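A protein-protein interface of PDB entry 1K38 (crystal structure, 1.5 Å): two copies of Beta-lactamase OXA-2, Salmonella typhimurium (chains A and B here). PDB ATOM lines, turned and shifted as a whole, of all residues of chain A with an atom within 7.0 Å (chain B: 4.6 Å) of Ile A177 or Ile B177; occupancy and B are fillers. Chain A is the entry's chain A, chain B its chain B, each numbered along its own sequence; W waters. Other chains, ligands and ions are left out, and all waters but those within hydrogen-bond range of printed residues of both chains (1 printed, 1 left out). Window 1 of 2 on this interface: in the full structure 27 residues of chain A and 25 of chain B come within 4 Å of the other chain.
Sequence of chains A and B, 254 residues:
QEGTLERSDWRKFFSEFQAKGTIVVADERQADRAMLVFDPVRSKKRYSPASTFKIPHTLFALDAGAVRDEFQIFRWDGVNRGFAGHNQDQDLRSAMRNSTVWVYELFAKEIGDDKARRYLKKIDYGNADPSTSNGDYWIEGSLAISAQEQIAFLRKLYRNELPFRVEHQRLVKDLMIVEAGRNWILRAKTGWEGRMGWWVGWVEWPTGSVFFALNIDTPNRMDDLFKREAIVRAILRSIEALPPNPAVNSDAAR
The guanidinium group (NH2) of Arg A93 lies within salt-bridge range of the side-chain carboxylate (OD2) of Asp A174. O of Lys B173 sits at hydrogen-bond distance from NH2 of Arg B187, 3.0 Å away. The backbone carbonyl oxygen (O) of Glu B179 lies within hydrogen-bond range of the backbone NH (N) of Leu B186 (2.8 Å). The backbone carbonyl oxygen of Leu B186 lies within hydrogen-bond range of the backbone NH of Val B178 (2.9 Å). O of Lys A173 sits at hydrogen-bond distance from NH2 of Arg A187 (3.0 Å). The backbone carbonyl oxygen of Glu A179 sits at hydrogen-bond distance from the backbone NH of Leu A186 (2.8 Å).
Among the printed residues, merely in contact across the chains: Ile A177 with Ile B177 (3.4 Å), Ala A180 with Glu B179 (3.4 Å), Glu A179 with Ala B180 (3.5 Å), Arg A93 with Ile B185 (3.5 Å), Arg A93 with Arg B187 (3.9 Å), Ala A180 with Ile B177 (3.9 Å), Ile A177 with Ala B180 (3.9 Å) and Arg A97 with Ile B185 (3.96 Å).
Of the printed residues of chain B, Arg A93 touches Ile B185 and Arg B187. Of chain B, only Ile B177 (3.4 Å) and Ala B180 (3.9 Å) come within 4 Å of Ile A177. Of the printed residues of chain B, Glu A179 touches Ala B180 (3.5 Å). Ala A188 touches none of the printed residues of chain B. Of the printed residues of chain A, Ile B177 touches Ile A177 (3.4 Å) and Ala A180 (3.9 Å). Of the printed residues of chain A, Ile B185 touches Arg A93 (3.5 Å) and Arg A97 (3.96 Å). The nearest residue of chain B that does not touch Ile A177 is Ile B185 (4.1 Å). The nearest printed residue of chain A that does not touch Ile B177 is Ile A185 (4.01 Å).
Asp A174 touches Arg B187, and with the chains exchanged Arg A187 touches Asp B174. Ile A177 touches Ala B180, and with the chains exchanged Ala A180 touches Ile B177. Glu A179 touches Ala B180, and with the chains exchanged Ala A180 touches Glu B179. Ala B180 touches its own counterpart, Ala A180. 11 positions are printed for both chains. Of the 13 pairs that touch across the chains among the printed residues, 8 have their exchanged pair printed and touching as well.
NH1 of Arg A187 lies within salt-bridge range of OD2 of Asp B174 (2.9 Å). The backbone carbonyl oxygen of Gly A181 lies close to the backbone carbonyl oxygen of Val B178 (3.2 Å). The guanidinium group (NH1) of Arg B187 lies within salt-bridge range of the side-chain carboxylate (OD2) of Asp A174 (2.8 Å). The backbone NH (N) of Arg A182 is in hydrogen-bond range of the backbone carbonyl oxygen (O) of Val B178, at 3.3 Å. The backbone NH (N) of Ala B180 lies within hydrogen-bond range of the backbone carbonyl oxygen (O) of Ala A180.
Hydrophobic or aromatic side chains of chain A within 4 Å of the printed part of chain B: Ile A177 and Ala A180. Of the 11 printed residues of chain B, 7 touch a printed residue of chain A. Hydrophobic or aromatic side chains of chain B within 4 Å of the printed part of chain A: Ile B177, Val B178, Ala B180 and Ile B185. Among the printed residues, 13 pairs touch across the chains. Among the printed residues, Asp or Glu carboxylates within 4 Å of a Lys or Arg side-chain nitrogen of the other chain: Asp A174 with Arg B187 and Arg A187 with Asp B174.
Water W1 lies within hydrogen-bond range of O of Gly A181 (2.8 Å) and O of Ile B177 (2.9 Å).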
ATOM      1  N   ARG A  93     -27.874  26.968  -5.342  1.00  0.00           N
ATOM      2  CA  ARG A  93     -26.677  26.982  -6.173  1.00  0.00           C
ATOM      3  C   ARG A  93     -26.690  28.098  -7.207  1.00  0.00           C
ATOM      4  O   ARG A  93     -25.668  28.745  -7.428  1.00  0.00           O
ATOM      5  CB  ARG A  93     -26.472  25.630  -6.861  1.00  0.00           C
ATOM      6  CG  ARG A  93     -25.032  25.420  -7.342  1.00  0.00           C
ATOM      7  CD  ARG A  93     -24.820  24.015  -7.894  1.00  0.00           C
ATOM      8  NE  ARG A  93     -25.030  22.973  -6.893  1.00  0.00           N
ATOM      9  CZ  ARG A  93     -24.100  22.542  -6.045  1.00  0.00           C
ATOM     10  NH1 ARG A  93     -22.879  23.061  -6.068  1.00  0.00           N
ATOM     11  NH2 ARG A  93     -24.393  21.587  -5.167  1.00  0.00           N
ATOM     12  N   MET A  96     -26.125  31.425  -5.416  1.00  0.00           N
ATOM     13  CA  MET A  96     -24.736  31.567  -5.002  1.00  0.00           C
ATOM     14  C   MET A  96     -23.860  31.912  -6.200  1.00  0.00           C
ATOM     15  O   MET A  96     -23.088  32.872  -6.170  1.00  0.00           O
ATOM     16  CB  MET A  96     -24.252  30.252  -4.384  1.00  0.00           C
ATOM     17  CG  MET A  96     -22.888  30.322  -3.725  1.00  0.00           C
ATOM     18  SD  MET A  96     -22.976  31.089  -2.102  1.00  0.00           S
ATOM     19  CE  MET A  96     -23.366  29.672  -1.077  1.00  0.00           C
ATOM     20  N   ARG A  97     -23.999  31.117  -7.254  1.00  0.00           N
ATOM     21  CA  ARG A  97     -23.223  31.273  -8.482  1.00  0.00           C
ATOM     22  C   ARG A  97     -23.446  32.622  -9.154  1.00  0.00           C
ATOM     23  O   ARG A  97     -22.516  33.204  -9.722  1.00  0.00           O
ATOM     24  CB  ARG A  97     -23.577  30.163  -9.475  1.00  0.00           C
ATOM     25  CG  ARG A  97     -22.981  28.799  -9.150  1.00  0.00           C
ATOM     26  CD  ARG A  97     -23.461  27.737 -10.132  1.00  0.00           C
ATOM     27  NE  ARG A  97     -22.723  26.480  -9.999  1.00  0.00           N
ATOM     28  CZ  ARG A  97     -23.070  25.345 -10.601  1.00  0.00           C
ATOM     29  NH1 ARG A  97     -24.151  25.303 -11.373  1.00  0.00           N
ATOM     30  NH2 ARG A  97     -22.327  24.253 -10.446  1.00  0.00           N
ATOM     31  N   VAL A 172     -22.749  24.287   2.033  1.00  0.00           N
ATOM     32  CA  VAL A 172     -22.215  25.569   1.596  1.00  0.00           C
ATOM     33  C   VAL A 172     -20.893  25.385   0.848  1.00  0.00           C
ATOM     34  O   VAL A 172     -20.670  26.029  -0.174  1.00  0.00           O
ATOM     35  CB  VAL A 172     -22.028  26.538   2.788  1.00  0.00           C
ATOM     36  CG1 VAL A 172     -21.276  27.790   2.338  1.00  0.00           C
ATOM     37  CG2 VAL A 172     -23.388  26.937   3.338  1.00  0.00           C
ATOM     38  N   LYS A 173     -20.018  24.509   1.338  1.00  0.00           N
ATOM     39  CA  LYS A 173     -18.746  24.291   0.647  1.00  0.00           C
ATOM     40  C   LYS A 173     -18.978  23.694  -0.736  1.00  0.00           C
ATOM     41  O   LYS A 173     -18.200  23.928  -1.664  1.00  0.00           O
ATOM     42  CB  LYS A 173     -17.814  23.405   1.486  1.00  0.00           C
ATOM     43  CG  LYS A 173     -17.195  24.168   2.650  1.00  0.00           C
ATOM     44  CD  LYS A 173     -16.215  23.325   3.462  1.00  0.00           C
ATOM     45  CE  LYS A 173     -16.932  22.309   4.337  1.00  0.00           C
ATOM     46  NZ  LYS A 173     -15.985  21.563   5.218  1.00  0.00           N
ATOM     47  N   ASP A 174     -20.052  22.930  -0.886  1.00  0.00           N
ATOM     48  CA  ASP A 174     -20.357  22.353  -2.183  1.00  0.00           C
ATOM     49  C   ASP A 174     -20.891  23.448  -3.114  1.00  0.00           C
ATOM     50  O   ASP A 174     -20.525  23.509  -4.286  1.00  0.00           O
ATOM     51  CB  ASP A 174     -21.375  21.225  -2.051  1.00  0.00           C
ATOM     52  CG  ASP A 174     -21.321  20.284  -3.228  1.00  0.00           C
ATOM     53  OD1 ASP A 174     -20.661  19.214  -3.134  1.00  0.00           O
ATOM     54  OD2 ASP A 174     -21.912  20.642  -4.259  1.00  0.00           O
ATOM     55  N   LEU A 175     -21.741  24.322  -2.587  1.00  0.00           N
ATOM     56  CA  LEU A 175     -22.301  25.415  -3.382  1.00  0.00           C
ATOM     57  C   LEU A 175     -21.202  26.348  -3.906  1.00  0.00           C
ATOM     58  O   LEU A 175     -21.347  26.962  -4.966  1.00  0.00           O
ATOM     59  CB  LEU A 175     -23.316  26.207  -2.541  1.00  0.00           C
ATOM     60  CG  LEU A 175     -24.572  25.431  -2.122  1.00  0.00           C
ATOM     61  CD1 LEU A 175     -25.382  26.254  -1.127  1.00  0.00           C
ATOM     62  CD2 LEU A 175     -25.408  25.103  -3.355  1.00  0.00           C
ATOM     63  N   MET A 176     -20.099  26.428  -3.166  1.00  0.00           N
ATOM     64  CA  MET A 176     -18.961  27.276  -3.524  1.00  0.00           C
ATOM     65  C   MET A 176     -18.086  26.734  -4.658  1.00  0.00           C
ATOM     66  O   MET A 176     -17.207  27.442  -5.152  1.00  0.00           O
ATOM     67  CB  MET A 176     -18.069  27.498  -2.297  1.00  0.00           C
ATOM     68  CG  MET A 176     -18.668  28.392  -1.218  1.00  0.00           C
ATOM     69  SD  MET A 176     -17.667  28.372   0.282  1.00  0.00           S
ATOM     70  CE  MET A 176     -16.119  29.076  -0.325  1.00  0.00           C
ATOM     71  N   ILE A 177     -18.311  25.494  -5.081  1.00  0.00           N
ATOM     72  CA  ILE A 177     -17.474  24.933  -6.139  1.00  0.00           C
ATOM     73  C   ILE A 177     -17.559  25.733  -7.431  1.00  0.00           C
ATOM     74  O   ILE A 177     -18.643  25.949  -7.975  1.00  0.00           O
ATOM     75  CB  ILE A 177     -17.840  23.466  -6.425  1.00  0.00           C
ATOM     76  CG1 ILE A 177     -17.557  22.616  -5.181  1.00  0.00           C
ATOM     77  CG2 ILE A 177     -17.032  22.946  -7.608  1.00  0.00           C
ATOM     78  CD1 ILE A 177     -18.196  21.239  -5.229  1.00  0.00           C
ATOM     79  N   VAL A 178     -16.396  26.156  -7.914  1.00  0.00           N
ATOM     80  CA  VAL A 178     -16.296  26.940  -9.141  1.00  0.00           C
ATOM     81  C   VAL A 178     -15.581  26.172 -10.247  1.00  0.00           C
ATOM     82  O   VAL A 178     -15.867  26.359 -11.431  1.00  0.00           O
ATOM     83  CB  VAL A 178     -15.533  28.266  -8.885  1.00  0.00           C
ATOM     84  CG1 VAL A 178     -15.288  29.002 -10.198  1.00  0.00           C
ATOM     85  CG2 VAL A 178     -16.336  29.143  -7.935  1.00  0.00           C
ATOM     86  N   GLU A 179     -14.659  25.300  -9.859  1.00  0.00           N
ATOM     87  CA  GLU A 179     -13.890  24.531 -10.828  1.00  0.00           C
ATOM     88  C   GLU A 179     -13.207  23.378 -10.108  1.00  0.00           C
ATOM     89  O   GLU A 179     -12.976  23.441  -8.902  1.00  0.00           O
ATOM     90  CB  GLU A 179     -12.826  25.437 -11.463  1.00  0.00           C
ATOM     91  CG  GLU A 179     -12.350  25.017 -12.838  1.00  0.00           C
ATOM     92  CD  GLU A 179     -11.357  26.008 -13.420  1.00  0.00           C
ATOM     93  OE1 GLU A 179     -11.566  27.227 -13.244  1.00  0.00           O
ATOM     94  OE2 GLU A 179     -10.378  25.571 -14.058  1.00  0.00           O
ATOM     95  N   ALA A 180     -12.881  22.322 -10.843  1.00  0.00           N
ATOM     96  CA  ALA A 180     -12.198  21.187 -10.241  1.00  0.00           C
ATOM     97  C   ALA A 180     -11.548  20.293 -11.283  1.00  0.00           C
ATOM     98  O   ALA A 180     -11.980  20.245 -12.437  1.00  0.00           O
ATOM     99  CB  ALA A 180     -13.170  20.366  -9.399  1.00  0.00           C
ATOM    100  N   GLY A 181     -10.492  19.611 -10.849  1.00  0.00           N
ATOM    101  CA  GLY A 181      -9.772  18.673 -11.687  1.00  0.00           C
ATOM    102  C   GLY A 181      -9.741  17.371 -10.907  1.00  0.00           C
ATOM    103  O   GLY A 181     -10.344  17.283  -9.842  1.00  0.00           O
ATOM    104  N   ARG A 182      -9.037  16.365 -11.413  1.00  0.00           N
ATOM    105  CA  ARG A 182      -8.971  15.082 -10.727  1.00  0.00           C
ATOM    106  C   ARG A 182      -8.417  15.154  -9.309  1.00  0.00           C
ATOM    107  O   ARG A 182      -8.860  14.410  -8.429  1.00  0.00           O
ATOM    108  CB  ARG A 182      -8.135  14.088 -11.543  1.00  0.00           C
ATOM    109  CG  ARG A 182      -8.761  13.689 -12.867  1.00  0.00           C
ATOM    110  CD  ARG A 182      -7.908  12.649 -13.579  1.00  0.00           C
ATOM    111  NE  ARG A 182      -8.453  12.303 -14.888  1.00  0.00           N
ATOM    112  CZ  ARG A 182      -9.586  11.633 -15.079  1.00  0.00           C
ATOM    113  NH1 ARG A 182     -10.308  11.224 -14.041  1.00  0.00           N
ATOM    114  NH2 ARG A 182     -10.005  11.381 -16.312  1.00  0.00           N
ATOM    115  N   ASN A 183      -7.457  16.048  -9.076  1.00  0.00           N
ATOM    116  CA  ASN A 183      -6.861  16.160  -7.750  1.00  0.00           C
ATOM    117  C   ASN A 183      -6.930  17.544  -7.112  1.00  0.00           C
ATOM    118  O   ASN A 183      -6.184  17.834  -6.178  1.00  0.00           O
ATOM    119  CB  ASN A 183      -5.399  15.692  -7.783  1.00  0.00           C
ATOM    120  CG  ASN A 183      -4.533  16.530  -8.697  1.00  0.00           C
ATOM    121  OD1 ASN A 183      -3.302  16.446  -8.649  1.00  0.00           O
ATOM    122  ND2 ASN A 183      -5.162  17.334  -9.541  1.00  0.00           N
ATOM    123  N   TRP A 184      -7.819  18.399  -7.602  1.00  0.00           N
ATOM    124  CA  TRP A 184      -7.951  19.731  -7.015  1.00  0.00           C
ATOM    125  C   TRP A 184      -9.369  20.281  -7.142  1.00  0.00           C
ATOM    126  O   TRP A 184     -10.069  20.000  -8.116  1.00  0.00           O
ATOM    127  CB  TRP A 184      -6.953  20.710  -7.645  1.00  0.00           C
ATOM    128  CG  TRP A 184      -7.126  20.928  -9.113  1.00  0.00           C
ATOM    129  CD1 TRP A 184      -6.638  20.149 -10.123  1.00  0.00           C
ATOM    130  CD2 TRP A 184      -7.848  21.992  -9.738  1.00  0.00           C
ATOM    131  NE1 TRP A 184      -7.011  20.665 -11.341  1.00  0.00           N
ATOM    132  CE2 TRP A 184      -7.755  21.796 -11.133  1.00  0.00           C
ATOM    133  CE3 TRP A 184      -8.566  23.094  -9.255  1.00  0.00           C
ATOM    134  CZ2 TRP A 184      -8.355  22.661 -12.052  1.00  0.00           C
ATOM    135  CZ3 TRP A 184      -9.163  23.953 -10.167  1.00  0.00           C
ATOM    136  CH2 TRP A 184      -9.055  23.732 -11.552  1.00  0.00           C
ATOM    137  N   ILE A 185      -9.785  21.052  -6.142  1.00  0.00           N
ATOM    138  CA  ILE A 185     -11.116  21.649  -6.131  1.00  0.00           C
ATOM    139  C   ILE A 185     -11.036  23.112  -5.722  1.00  0.00           C
ATOM    140  O   ILE A 185     -10.495  23.446  -4.668  1.00  0.00           O
ATOM    141  CB  ILE A 185     -12.062  20.917  -5.141  1.00  0.00           C
ATOM    142  CG1 ILE A 185     -12.168  19.438  -5.523  1.00  0.00           C
ATOM    143  CG2 ILE A 185     -13.456  21.551  -5.178  1.00  0.00           C
ATOM    144  CD1 ILE A 185     -12.962  18.598  -4.539  1.00  0.00           C
ATOM    145  N   LEU A 186     -11.577  23.983  -6.565  1.00  0.00           N
ATOM    146  CA  LEU A 186     -11.581  25.414  -6.289  1.00  0.00           C
ATOM    147  C   LEU A 186     -12.954  25.808  -5.772  1.00  0.00           C
ATOM    148  O   LEU A 186     -13.957  25.619  -6.466  1.00  0.00           O
ATOM    149  CB  LEU A 186     -11.264  26.206  -7.566  1.00  0.00           C
ATOM    150  CG  LEU A 186     -11.406  27.735  -7.499  1.00  0.00           C
ATOM    151  CD1 LEU A 186     -10.394  28.326  -6.519  1.00  0.00           C
ATOM    152  CD2 LEU A 186     -11.187  28.322  -8.893  1.00  0.00           C
ATOM    153  N   ARG A 187     -12.992  26.337  -4.549  1.00  0.00           N
ATOM    154  CA  ARG A 187     -14.236  26.778  -3.921  1.00  0.00           C
ATOM    155  C   ARG A 187     -14.070  28.264  -3.657  1.00  0.00           C
ATOM    156  O   ARG A 187     -13.121  28.677  -2.987  1.00  0.00           O
ATOM    157  CB  ARG A 187     -14.474  26.038  -2.598  1.00  0.00           C
ATOM    158  CG  ARG A 187     -14.400  24.513  -2.698  1.00  0.00           C
ATOM    159  CD  ARG A 187     -14.758  23.878  -1.357  1.00  0.00           C
ATOM    160  NE  ARG A 187     -14.324  22.484  -1.267  1.00  0.00           N
ATOM    161  CZ  ARG A 187     -15.065  21.426  -1.579  1.00  0.00           C
ATOM    162  NH1 ARG A 187     -14.546  20.208  -1.457  1.00  0.00           N
ATOM    163  NH2 ARG A 187     -16.319  21.575  -1.999  1.00  0.00           N
ATOM    164  N   ALA A 188     -14.981  29.078  -4.177  1.00  0.00           N
ATOM    165  CA  ALA A 188     -14.850  30.514  -3.981  1.00  0.00           C
ATOM    166  C   ALA A 188     -16.153  31.278  -4.128  1.00  0.00           C
ATOM    167  O   ALA A 188     -17.178  30.724  -4.520  1.00  0.00           O
ATOM    168  CB  ALA A 188     -13.821  31.057  -4.960  1.00  0.00           C
ATOM    169  N   LYS B 173     -20.636  12.675  -1.606  1.00  0.00           N
ATOM    170  CA  LYS B 173     -20.835  13.337  -2.894  1.00  0.00           C
ATOM    171  C   LYS B 173     -19.675  14.291  -3.192  1.00  0.00           C
ATOM    172  O   LYS B 173     -19.310  14.498  -4.353  1.00  0.00           O
ATOM    173  CB  LYS B 173     -22.183  14.072  -2.919  1.00  0.00           C
ATOM    174  CG  LYS B 173     -23.356  13.121  -3.125  1.00  0.00           C
ATOM    175  CD  LYS B 173     -24.694  13.831  -3.231  1.00  0.00           C
ATOM    176  CE  LYS B 173     -25.189  14.309  -1.876  1.00  0.00           C
ATOM    177  NZ  LYS B 173     -26.558  14.885  -1.999  1.00  0.00           N
ATOM    178  N   ASP B 174     -19.096  14.856  -2.135  1.00  0.00           N
ATOM    179  CA  ASP B 174     -17.946  15.757  -2.225  1.00  0.00           C
ATOM    180  C   ASP B 174     -16.729  14.923  -2.664  1.00  0.00           C
ATOM    181  O   ASP B 174     -16.006  15.287  -3.595  1.00  0.00           O
ATOM    182  CB  ASP B 174     -17.717  16.382  -0.831  1.00  0.00           C
ATOM    183  CG  ASP B 174     -16.444  17.232  -0.728  1.00  0.00           C
ATOM    184  OD1 ASP B 174     -16.017  17.483   0.422  1.00  0.00           O
ATOM    185  OD2 ASP B 174     -15.877  17.662  -1.747  1.00  0.00           O
ATOM    186  N   LEU B 175     -16.519  13.792  -1.998  1.00  0.00           N
ATOM    187  CA  LEU B 175     -15.390  12.914  -2.306  1.00  0.00           C
ATOM    188  C   LEU B 175     -15.419  12.388  -3.740  1.00  0.00           C
ATOM    189  O   LEU B 175     -14.373  12.087  -4.319  1.00  0.00           O
ATOM    190  CB  LEU B 175     -15.368  11.736  -1.327  1.00  0.00           C
ATOM    191  CG  LEU B 175     -15.196  12.120   0.145  1.00  0.00           C
ATOM    192  CD1 LEU B 175     -15.455  10.903   1.021  1.00  0.00           C
ATOM    193  CD2 LEU B 175     -13.789  12.659   0.381  1.00  0.00           C
ATOM    194  N   MET B 176     -16.616  12.300  -4.310  1.00  0.00           N
ATOM    195  CA  MET B 176     -16.805  11.796  -5.667  1.00  0.00           C
ATOM    196  C   MET B 176     -16.466  12.793  -6.767  1.00  0.00           C
ATOM    197  O   MET B 176     -16.439  12.428  -7.935  1.00  0.00           O
ATOM    198  CB  MET B 176     -18.256  11.346  -5.861  1.00  0.00           C
ATOM    199  CG  MET B 176     -18.631  10.048  -5.162  1.00  0.00           C
ATOM    200  SD  MET B 176     -20.410   9.766  -5.211  1.00  0.00           S
ATOM    201  CE  MET B 176     -20.653   9.509  -6.972  1.00  0.00           C
ATOM    202  N   ILE B 177     -16.216  14.047  -6.409  1.00  0.00           N
ATOM    203  CA  ILE B 177     -15.916  15.051  -7.428  1.00  0.00           C
ATOM    204  C   ILE B 177     -14.678  14.699  -8.238  1.00  0.00           C
ATOM    205  O   ILE B 177     -13.599  14.489  -7.688  1.00  0.00           O
ATOM    206  CB  ILE B 177     -15.730  16.440  -6.810  1.00  0.00           C
ATOM    207  CG1 ILE B 177     -17.034  16.894  -6.153  1.00  0.00           C
ATOM    208  CG2 ILE B 177     -15.322  17.436  -7.898  1.00  0.00           C
ATOM    209  CD1 ILE B 177     -16.876  18.085  -5.233  1.00  0.00           C
ATOM    210  N   VAL B 178     -14.854  14.642  -9.553  1.00  0.00           N
ATOM    211  CA  VAL B 178     -13.776  14.310 -10.478  1.00  0.00           C
ATOM    212  C   VAL B 178     -13.379  15.494 -11.348  1.00  0.00           C
ATOM    213  O   VAL B 178     -12.227  15.616 -11.755  1.00  0.00           O
ATOM    214  CB  VAL B 178     -14.195  13.130 -11.391  1.00  0.00           C
ATOM    215  CG1 VAL B 178     -13.196  12.945 -12.528  1.00  0.00           C
ATOM    216  CG2 VAL B 178     -14.280  11.858 -10.561  1.00  0.00           C
ATOM    217  N   GLU B 179     -14.335  16.369 -11.623  1.00  0.00           N
ATOM    218  CA  GLU B 179     -14.084  17.525 -12.470  1.00  0.00           C
ATOM    219  C   GLU B 179     -15.259  18.480 -12.320  1.00  0.00           C
ATOM    220  O   GLU B 179     -16.360  18.064 -11.960  1.00  0.00           O
ATOM    221  CB  GLU B 179     -13.957  17.044 -13.921  1.00  0.00           C
ATOM    222  CG  GLU B 179     -13.588  18.090 -14.947  1.00  0.00           C
ATOM    223  CD  GLU B 179     -13.454  17.487 -16.337  1.00  0.00           C
ATOM    224  OE1 GLU B 179     -13.988  16.379 -16.560  1.00  0.00           O
ATOM    225  OE2 GLU B 179     -12.822  18.116 -17.206  1.00  0.00           O
ATOM    226  N   ALA B 180     -15.031  19.764 -12.589  1.00  0.00           N
ATOM    227  CA  ALA B 180     -16.104  20.738 -12.485  1.00  0.00           C
ATOM    228  C   ALA B 180     -15.814  22.021 -13.239  1.00  0.00           C
ATOM    229  O   ALA B 180     -14.655  22.387 -13.458  1.00  0.00           O
ATOM    230  CB  ALA B 180     -16.387  21.065 -11.017  1.00  0.00           C
ATOM    231  N   ILE B 185     -20.843  20.019 -12.425  1.00  0.00           N
ATOM    232  CA  ILE B 185     -20.002  19.238 -11.526  1.00  0.00           C
ATOM    233  C   ILE B 185     -20.139  17.757 -11.851  1.00  0.00           C
ATOM    234  O   ILE B 185     -21.245  17.221 -11.870  1.00  0.00           O
ATOM    235  CB  ILE B 185     -20.414  19.444 -10.051  1.00  0.00           C
ATOM    236  CG1 ILE B 185     -20.327  20.925  -9.681  1.00  0.00           C
ATOM    237  CG2 ILE B 185     -19.517  18.612  -9.135  1.00  0.00           C
ATOM    238  CD1 ILE B 185     -20.874  21.231  -8.292  1.00  0.00           C
ATOM    239  N   LEU B 186     -19.010  17.105 -12.112  1.00  0.00           N
ATOM    240  CA  LEU B 186     -18.991  15.678 -12.420  1.00  0.00           C
ATOM    241  C   LEU B 186     -18.563  14.897 -11.180  1.00  0.00           C
ATOM    242  O   LEU B 186     -17.464  15.098 -10.666  1.00  0.00           O
ATOM    243  CB  LEU B 186     -18.011  15.397 -13.565  1.00  0.00           C
ATOM    244  CG  LEU B 186     -17.670  13.935 -13.876  1.00  0.00           C
ATOM    245  CD1 LEU B 186     -18.908  13.173 -14.329  1.00  0.00           C
ATOM    246  CD2 LEU B 186     -16.597  13.908 -14.960  1.00  0.00           C
ATOM    247  N   ARG B 187     -19.450  14.028 -10.696  1.00  0.00           N
ATOM    248  CA  ARG B 187     -19.183  13.200  -9.518  1.00  0.00           C
ATOM    249  C   ARG B 187     -19.209  11.759 -10.012  1.00  0.00           C
ATOM    250  O   ARG B 187     -20.196  11.331 -10.597  1.00  0.00           O
ATOM    251  CB  ARG B 187     -20.273  13.408  -8.460  1.00  0.00           C
ATOM    252  CG  ARG B 187     -20.475  14.870  -8.049  1.00  0.00           C
ATOM    253  CD  ARG B 187     -21.516  14.992  -6.934  1.00  0.00           C
ATOM    254  NE  ARG B 187     -22.063  16.343  -6.827  1.00  0.00           N
ATOM    255  CZ  ARG B 187     -21.593  17.300  -6.030  1.00  0.00           C
ATOM    256  NH1 ARG B 187     -22.176  18.494  -6.024  1.00  0.00           N
ATOM    257  NH2 ARG B 187     -20.559  17.071  -5.229  1.00  0.00           N
HETATM  258  O   HOH W   1     -11.589  16.556  -7.455  1.00  0.00           O
